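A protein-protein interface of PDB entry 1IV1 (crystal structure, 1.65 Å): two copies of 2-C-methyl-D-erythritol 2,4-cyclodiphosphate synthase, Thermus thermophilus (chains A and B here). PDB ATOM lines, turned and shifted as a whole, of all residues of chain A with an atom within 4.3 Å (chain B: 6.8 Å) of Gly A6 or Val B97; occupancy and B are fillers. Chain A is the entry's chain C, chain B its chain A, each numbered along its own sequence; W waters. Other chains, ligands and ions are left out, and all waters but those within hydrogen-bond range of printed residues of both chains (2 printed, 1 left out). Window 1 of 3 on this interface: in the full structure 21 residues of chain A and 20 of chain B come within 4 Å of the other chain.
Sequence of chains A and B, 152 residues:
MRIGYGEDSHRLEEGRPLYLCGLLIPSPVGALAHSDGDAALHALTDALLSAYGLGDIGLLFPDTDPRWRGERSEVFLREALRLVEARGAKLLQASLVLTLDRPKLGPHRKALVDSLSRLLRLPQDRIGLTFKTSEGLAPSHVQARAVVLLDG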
ATOM      1  N   TYR A   5     -27.142  15.253 -29.616  1.00  0.00           N
ATOM      2  CA  TYR A   5     -27.016  16.390 -28.715  1.00  0.00           C
ATOM      3  C   TYR A   5     -27.032  17.682 -29.519  1.00  0.00           C
ATOM      4  O   TYR A   5     -26.327  17.784 -30.525  1.00  0.00           O
ATOM      5  CB  TYR A   5     -25.736  16.259 -27.885  1.00  0.00           C
ATOM      6  CG  TYR A   5     -25.486  17.489 -27.049  1.00  0.00           C
ATOM      7  CD1 TYR A   5     -26.194  17.695 -25.869  1.00  0.00           C
ATOM      8  CD2 TYR A   5     -24.549  18.430 -27.458  1.00  0.00           C
ATOM      9  CE1 TYR A   5     -25.977  18.817 -25.093  1.00  0.00           C
ATOM     10  CE2 TYR A   5     -24.334  19.560 -26.675  1.00  0.00           C
ATOM     11  CZ  TYR A   5     -25.044  19.739 -25.511  1.00  0.00           C
ATOM     12  OH  TYR A   5     -24.818  20.868 -24.756  1.00  0.00           O
ATOM     13  N   GLY A   6     -27.826  18.687 -29.136  1.00  0.00           N
ATOM     14  CA  GLY A   6     -27.887  19.896 -29.965  1.00  0.00           C
ATOM     15  C   GLY A   6     -27.998  21.154 -29.103  1.00  0.00           C
ATOM     16  O   GLY A   6     -28.496  21.040 -27.985  1.00  0.00           O
ATOM     17  N   GLU A   7     -27.550  22.306 -29.586  1.00  0.00           N
ATOM     18  CA  GLU A   7     -27.651  23.521 -28.782  1.00  0.00           C
ATOM     19  C   GLU A   7     -28.087  24.658 -29.700  1.00  0.00           C
ATOM     20  O   GLU A   7     -27.786  24.648 -30.882  1.00  0.00           O
ATOM     21  CB  GLU A   7     -26.364  24.019 -28.152  1.00  0.00           C
ATOM     22  CG  GLU A   7     -25.603  23.158 -27.184  1.00  0.00           C
ATOM     23  CD  GLU A   7     -24.332  23.836 -26.683  1.00  0.00           C
ATOM     24  OE1 GLU A   7     -24.402  24.977 -26.178  1.00  0.00           O
ATOM     25  OE2 GLU A   7     -23.262  23.222 -26.800  1.00  0.00           O
ATOM     26  N   ALA A  43     -32.570  23.623 -31.039  1.00  0.00           N
ATOM     27  CA  ALA A  43     -31.691  22.641 -30.416  1.00  0.00           C
ATOM     28  C   ALA A  43     -32.215  21.222 -30.583  1.00  0.00           C
ATOM     29  O   ALA A  43     -31.425  20.289 -30.773  1.00  0.00           O
ATOM     30  CB  ALA A  43     -31.501  22.907 -28.928  1.00  0.00           C
ATOM     31  N   ASP A  46     -31.469  20.137 -34.305  1.00  0.00           N
ATOM     32  CA  ASP A  46     -30.051  19.828 -34.425  1.00  0.00           C
ATOM     33  C   ASP A  46     -29.736  18.489 -33.775  1.00  0.00           C
ATOM     34  O   ASP A  46     -28.943  17.703 -34.308  1.00  0.00           O
ATOM     35  CB  ASP A  46     -29.234  20.951 -33.787  1.00  0.00           C
ATOM     36  CG  ASP A  46     -28.788  21.974 -34.822  1.00  0.00           C
ATOM     37  OD1 ASP A  46     -29.163  21.828 -36.004  1.00  0.00           O
ATOM     38  OD2 ASP A  46     -28.065  22.925 -34.481  1.00  0.00           O
ATOM     39  N   ALA A  47     -30.312  18.201 -32.615  1.00  0.00           N
ATOM     40  CA  ALA A  47     -30.025  16.924 -31.929  1.00  0.00           C
ATOM     41  C   ALA A  47     -30.463  15.722 -32.755  1.00  0.00           C
ATOM     42  O   ALA A  47     -29.727  14.730 -32.875  1.00  0.00           O
ATOM     43  CB  ALA A  47     -30.691  16.906 -30.568  1.00  0.00           C
ATOM     44  N   ALA A 144     -30.660  27.063 -25.425  1.00  0.00           N
ATOM     45  CA  ALA A 144     -31.323  25.773 -25.359  1.00  0.00           C
ATOM     46  C   ALA A 144     -30.280  24.670 -25.639  1.00  0.00           C
ATOM     47  O   ALA A 144     -29.501  24.855 -26.564  1.00  0.00           O
ATOM     48  CB  ALA A 144     -32.479  25.598 -26.318  1.00  0.00           C
ATOM     49  N   ARG A 145     -30.355  23.633 -24.829  1.00  0.00           N
ATOM     50  CA  ARG A 145     -29.496  22.450 -25.028  1.00  0.00           C
ATOM     51  C   ARG A 145     -30.345  21.199 -24.891  1.00  0.00           C
ATOM     52  O   ARG A 145     -31.125  21.063 -23.941  1.00  0.00           O
ATOM     53  CB  ARG A 145     -28.365  22.477 -24.013  1.00  0.00           C
ATOM     54  CG  ARG A 145     -27.299  23.478 -24.377  1.00  0.00           C
ATOM     55  CD  ARG A 145     -26.342  23.778 -23.229  1.00  0.00           C
ATOM     56  NE  ARG A 145     -25.567  24.957 -23.662  1.00  0.00           N
ATOM     57  CZ  ARG A 145     -25.661  26.098 -22.995  1.00  0.00           C
ATOM     58  NH1 ARG A 145     -26.454  26.124 -21.931  1.00  0.00           N
ATOM     59  NH2 ARG A 145     -24.960  27.140 -23.411  1.00  0.00           N
ATOM     60  N   ALA A 146     -30.216  20.271 -25.830  1.00  0.00           N
ATOM     61  CA  ALA A 146     -31.102  19.122 -25.846  1.00  0.00           C
ATOM     62  C   ALA A 146     -30.367  17.819 -26.145  1.00  0.00           C
ATOM     63  O   ALA A 146     -29.421  17.854 -26.943  1.00  0.00           O
ATOM     64  CB  ALA A 146     -32.175  19.357 -26.918  1.00  0.00           C
ATOM     65  N   ALA B  43     -13.277  18.021 -25.473  1.00  0.00           N
ATOM     66  CA  ALA B  43     -14.595  17.603 -25.006  1.00  0.00           C
ATOM     67  C   ALA B  43     -14.837  16.112 -25.254  1.00  0.00           C
ATOM     68  O   ALA B  43     -15.359  15.403 -24.384  1.00  0.00           O
ATOM     69  CB  ALA B  43     -15.679  18.431 -25.703  1.00  0.00           C
ATOM     70  N   SER B  95     -21.738  12.607 -30.415  1.00  0.00           N
ATOM     71  CA  SER B  95     -22.498  13.767 -30.919  1.00  0.00           C
ATOM     72  C   SER B  95     -21.986  15.029 -30.251  1.00  0.00           C
ATOM     73  O   SER B  95     -21.967  15.120 -29.022  1.00  0.00           O
ATOM     74  CB  SER B  95     -23.971  13.493 -30.653  1.00  0.00           C
ATOM     75  OG  SER B  95     -24.804  14.523 -31.174  1.00  0.00           O
ATOM     76  N   LEU B  96     -21.554  16.035 -31.015  1.00  0.00           N
ATOM     77  CA  LEU B  96     -21.024  17.234 -30.376  1.00  0.00           C
ATOM     78  C   LEU B  96     -21.378  18.516 -31.129  1.00  0.00           C
ATOM     79  O   LEU B  96     -21.632  18.533 -32.321  1.00  0.00           O
ATOM     80  CB  LEU B  96     -19.505  17.161 -30.232  1.00  0.00           C
ATOM     81  CG  LEU B  96     -18.679  17.089 -31.519  1.00  0.00           C
ATOM     82  CD1 LEU B  96     -17.240  17.514 -31.252  1.00  0.00           C
ATOM     83  CD2 LEU B  96     -18.720  15.697 -32.130  1.00  0.00           C
ATOM     84  N   VAL B  97     -21.337  19.604 -30.356  1.00  0.00           N
ATOM     85  CA  VAL B  97     -21.654  20.917 -30.879  1.00  0.00           C
ATOM     86  C   VAL B  97     -20.498  21.879 -30.668  1.00  0.00           C
ATOM     87  O   VAL B  97     -19.993  21.969 -29.549  1.00  0.00           O
ATOM     88  CB  VAL B  97     -22.911  21.512 -30.194  1.00  0.00           C
ATOM     89  CG1 VAL B  97     -23.256  22.853 -30.826  1.00  0.00           C
ATOM     90  CG2 VAL B  97     -24.071  20.540 -30.285  1.00  0.00           C
ATOM     91  N   LEU B  98     -20.115  22.559 -31.735  1.00  0.00           N
ATOM     92  CA  LEU B  98     -19.074  23.575 -31.711  1.00  0.00           C
ATOM     93  C   LEU B  98     -19.719  24.947 -31.869  1.00  0.00           C
ATOM     94  O   LEU B  98     -20.492  25.208 -32.785  1.00  0.00           O
ATOM     95  CB  LEU B  98     -18.029  23.325 -32.795  1.00  0.00           C
ATOM     96  CG  LEU B  98     -17.457  21.911 -32.878  1.00  0.00           C
ATOM     97  CD1 LEU B  98     -16.387  21.795 -33.956  1.00  0.00           C
ATOM     98  CD2 LEU B  98     -16.863  21.494 -31.538  1.00  0.00           C
ATOM     99  N   THR B  99     -19.364  25.808 -30.926  1.00  0.00           N
ATOM    100  CA  THR B  99     -19.892  27.166 -30.853  1.00  0.00           C
ATOM    101  C   THR B  99     -18.748  28.168 -30.932  1.00  0.00           C
ATOM    102  O   THR B  99     -17.835  28.216 -30.102  1.00  0.00           O
ATOM    103  CB  THR B  99     -20.721  27.317 -29.565  1.00  0.00           C
ATOM    104  OG1 THR B  99     -21.768  26.337 -29.558  1.00  0.00           O
ATOM    105  CG2 THR B  99     -21.430  28.663 -29.494  1.00  0.00           C
ATOM    106  N   GLY B 128     -22.006  12.861 -35.010  1.00  0.00           N
ATOM    107  CA  GLY B 128     -22.997  13.934 -35.014  1.00  0.00           C
ATOM    108  C   GLY B 128     -22.315  15.247 -34.705  1.00  0.00           C
ATOM    109  O   GLY B 128     -22.064  15.582 -33.540  1.00  0.00           O
ATOM    110  N   LEU B 129     -21.995  15.989 -35.750  1.00  0.00           N
ATOM    111  CA  LEU B 129     -21.294  17.257 -35.615  1.00  0.00           C
ATOM    112  C   LEU B 129     -22.171  18.439 -36.038  1.00  0.00           C
ATOM    113  O   LEU B 129     -22.627  18.453 -37.179  1.00  0.00           O
ATOM    114  CB  LEU B 129     -20.050  17.249 -36.502  1.00  0.00           C
ATOM    115  CG  LEU B 129     -19.215  18.524 -36.504  1.00  0.00           C
ATOM    116  CD1 LEU B 129     -18.885  18.929 -35.070  1.00  0.00           C
ATOM    117  CD2 LEU B 129     -17.944  18.339 -37.325  1.00  0.00           C
ATOM    118  N   THR B 130     -22.401  19.413 -35.156  1.00  0.00           N
ATOM    119  CA  THR B 130     -23.131  20.606 -35.598  1.00  0.00           C
ATOM    120  C   THR B 130     -22.339  21.865 -35.247  1.00  0.00           C
ATOM    121  O   THR B 130     -21.527  21.813 -34.317  1.00  0.00           O
ATOM    122  CB  THR B 130     -24.549  20.639 -34.994  1.00  0.00           C
ATOM    123  OG1 THR B 130     -24.475  20.729 -33.567  1.00  0.00           O
ATOM    124  CG2 THR B 130     -25.270  19.349 -35.346  1.00  0.00           C
ATOM    125  N   PHE B 131     -22.553  22.961 -35.965  1.00  0.00           N
ATOM    126  CA  PHE B 131     -21.860  24.223 -35.841  1.00  0.00           C
ATOM    127  C   PHE B 131     -22.835  25.345 -35.473  1.00  0.00           C
ATOM    128  O   PHE B 131     -23.876  25.466 -36.106  1.00  0.00           O
ATOM    129  CB  PHE B 131     -21.132  24.655 -37.116  1.00  0.00           C
ATOM    130  CG  PHE B 131     -20.217  23.606 -37.732  1.00  0.00           C
ATOM    131  CD1 PHE B 131     -19.392  22.832 -36.931  1.00  0.00           C
ATOM    132  CD2 PHE B 131     -20.209  23.417 -39.105  1.00  0.00           C
ATOM    133  CE1 PHE B 131     -18.559  21.869 -37.484  1.00  0.00           C
ATOM    134  CE2 PHE B 131     -19.384  22.463 -39.670  1.00  0.00           C
ATOM    135  CZ  PHE B 131     -18.570  21.695 -38.854  1.00  0.00           C
ATOM    136  N   LYS B 132     -22.468  26.134 -34.474  1.00  0.00           N
ATOM    137  CA  LYS B 132     -23.313  27.263 -34.082  1.00  0.00           C
ATOM    138  C   LYS B 132     -22.512  28.533 -33.866  1.00  0.00           C
ATOM    139  O   LYS B 132     -21.307  28.472 -33.622  1.00  0.00           O
ATOM    140  CB  LYS B 132     -24.030  26.945 -32.764  1.00  0.00           C
ATOM    141  CG  LYS B 132     -24.828  25.659 -32.741  1.00  0.00           C
ATOM    142  CD  LYS B 132     -25.857  25.610 -33.854  1.00  0.00           C
ATOM    143  CE  LYS B 132     -27.276  25.815 -33.372  1.00  0.00           C
ATOM    144  NZ  LYS B 132     -27.776  27.186 -33.722  1.00  0.00           N
ATOM    145  N   GLN B 143     -16.248  27.032 -27.967  1.00  0.00           N
ATOM    146  CA  GLN B 143     -16.824  26.098 -27.012  1.00  0.00           C
ATOM    147  C   GLN B 143     -17.183  24.785 -27.716  1.00  0.00           C
ATOM    148  O   GLN B 143     -17.581  24.849 -28.879  1.00  0.00           O
ATOM    149  CB  GLN B 143     -18.080  26.627 -26.330  1.00  0.00           C
ATOM    150  CG  GLN B 143     -18.015  28.083 -25.894  1.00  0.00           C
ATOM    151  CD  GLN B 143     -19.386  28.644 -25.537  1.00  0.00           C
ATOM    152  OE1 GLN B 143     -19.970  29.492 -26.213  1.00  0.00           O
ATOM    153  NE2 GLN B 143     -19.931  28.169 -24.421  1.00  0.00           N
ATOM    154  N   ALA B 144     -17.045  23.676 -27.008  1.00  0.00           N
ATOM    155  CA  ALA B 144     -17.478  22.361 -27.454  1.00  0.00           C
ATOM    156  C   ALA B 144     -18.159  21.612 -26.308  1.00  0.00           C
ATOM    157  O   ALA B 144     -17.664  21.665 -25.178  1.00  0.00           O
ATOM    158  CB  ALA B 144     -16.332  21.505 -27.981  1.00  0.00           C
ATOM    159  N   ARG B 145     -19.250  20.934 -26.631  1.00  0.00           N
ATOM    160  CA  ARG B 145     -19.948  20.028 -25.735  1.00  0.00           C
ATOM    161  C   ARG B 145     -20.221  18.713 -26.472  1.00  0.00           C
ATOM    162  O   ARG B 145     -20.746  18.726 -27.584  1.00  0.00           O
ATOM    163  CB  ARG B 145     -21.277  20.578 -25.242  1.00  0.00           C
ATOM    164  CG  ARG B 145     -21.226  21.236 -23.881  1.00  0.00           C
ATOM    165  CD  ARG B 145     -22.208  22.403 -23.800  1.00  0.00           C
ATOM    166  NE  ARG B 145     -21.487  23.557 -23.297  1.00  0.00           N
ATOM    167  CZ  ARG B 145     -21.411  24.768 -23.813  1.00  0.00           C
ATOM    168  NH1 ARG B 145     -22.042  25.086 -24.927  1.00  0.00           N
ATOM    169  NH2 ARG B 145     -20.670  25.651 -23.155  1.00  0.00           N
ATOM    170  N   ALA B 146     -19.845  17.623 -25.811  1.00  0.00           N
ATOM    171  CA  ALA B 146     -19.951  16.336 -26.490  1.00  0.00           C
ATOM    172  C   ALA B 146     -20.607  15.269 -25.627  1.00  0.00           C
ATOM    173  O   ALA B 146     -20.349  15.154 -24.436  1.00  0.00           O
ATOM    174  CB  ALA B 146     -18.558  15.883 -26.938  1.00  0.00           C
ATOM    175  N   VAL B 147     -21.420  14.453 -26.275  1.00  0.00           N
ATOM    176  CA  VAL B 147     -21.964  13.229 -25.716  1.00  0.00           C
ATOM    177  C   VAL B 147     -21.438  12.010 -26.470  1.00  0.00           C
ATOM    178  O   VAL B 147     -21.384  12.086 -27.699  1.00  0.00           O
ATOM    179  CB  VAL B 147     -23.498  13.257 -25.798  1.00  0.00           C
ATOM    180  CG1 VAL B 147     -24.073  11.968 -25.247  1.00  0.00           C
ATOM    181  CG2 VAL B 147     -24.011  14.475 -25.042  1.00  0.00           C
HETATM  182  O   HOH W   1     -21.105  24.257 -27.994  1.00  0.00           O
HETATM  183  O   HOH W   2     -26.635  22.420 -32.397  1.00  0.00           O
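Arg B145 touches its own counterpart, Arg A145.
The guanidinium group of Arg B145 is in salt-bridge range of the side-chain carboxylate of Glu A7.
The backbone NH (N) of Tyr A5 is in hydrogen-bond range of the side-chain hydroxyl (OG) of Ser B95 (2.9 Å).
Among the printed residues, pairs that only touch across the chains: Glu A7 with Lys B132 (2.8 Å), Tyr A5 with Arg B145 (3.2 Å), Asp A46 with Lys B132 (3.2 Å), Tyr A5 with Val B97 (3.6 Å), Arg A145 with Arg B145 (3.7 Å), Tyr A5 with Val B147 (3.8 Å), Glu A7 with Val B97 (3.8 Å) and Gly A6 with Val B97 (3.9 Å).
Of the 9 printed residues of chain A, 5 touch a printed residue of chain B.
Of the 16 printed residues of chain B, 5 touch a printed residue of chain A.
Printed residues of chain B that touch a printed residue of chain A: Ser B95, Val B97, Lys B132, Arg B145 and Val B147.
Hydrophobic or aromatic side chains of chain B within 4 Å of the printed part of chain A: Val B97 and Val B147.
Along chain B the printed residues that touch a printed residue of chain A span positions 95 to 147.
Among the printed residues, Asp or Glu carboxylates within 4 Å of a Lys or Arg side-chain nitrogen of the other chain: Glu A7 with Arg B145.
O of Ala A146 sits at hydrogen-bond distance from N of Gly A6, at 2.8 Å.
The backbone carbonyl oxygen (O) of Val B147 is in hydrogen-bond range of the backbone NH (N) of Ser B95, at 2.8 Å.
The side-chain amide nitrogen of Gln B143 lies close to the guanidinium group of Arg B145 (2.9 Å).
The backbone carbonyl oxygen of Leu B98 lies within hydrogen-bond range of the backbone NH of Lys B132, 2.8 Å away.
The backbone NH (N) of Val B97 sits at hydrogen-bond distance from the backbone carbonyl oxygen (O) of Arg B145 (3.0 Å).
OE2 of Glu A7 sits close to OH of Tyr A5.
Water W2 lies within hydrogen-bond range of OD2 of Asp A46 (2.6 Å), O of Glu A7 (2.9 Å) and OG1 of Thr B130 (3.0 Å).
Water W1 lies within hydrogen-bond range of the side-chain carboxylate (OE2) of Glu A7 (2.7 Å), the side-chain hydroxyl (OG1) of Thr B99 (2.7 Å), the backbone carbonyl oxygen (O) of Val B97 (3.0 Å) and the guanidinium group (NH1) of Arg B145 (3.3 Å).
Printed residues of chain B within 4 Å of Gly A6: Val B97.
Printed residues of chain B within 4 Å of Glu A7: Val B97 (3.8 Å), Lys B132 (2.8 Å) and Arg B145 (2.7 Å).
Printed residues of chain B within 4 Å of Asp A46: Lys B132.
Printed residues of chain B within 4 Å of Arg A145: Arg B145 (3.7 Å).
Of the printed residues of chain A, Ser B95 touches Tyr A5 (2.9 Å).
Leu B96 touches none of the printed residues of chain A.
Val B97 touches just these residues of chain A: Tyr A5 (3.6 Å), Gly A6 (3.9 Å) and Glu A7 (3.8 Å).
Ala B144 touches none of the printed residues of chain A.
Of the printed residues of chain A, Arg B145 touches Tyr A5, Glu A7 and Arg A145.
The nearest residue of chain B that does not touch Gly A6 is Thr B130 (5.0 Å).
The nearest printed residue of chain A that does not touch Val B97 is Asp A46 (6.0 Å).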
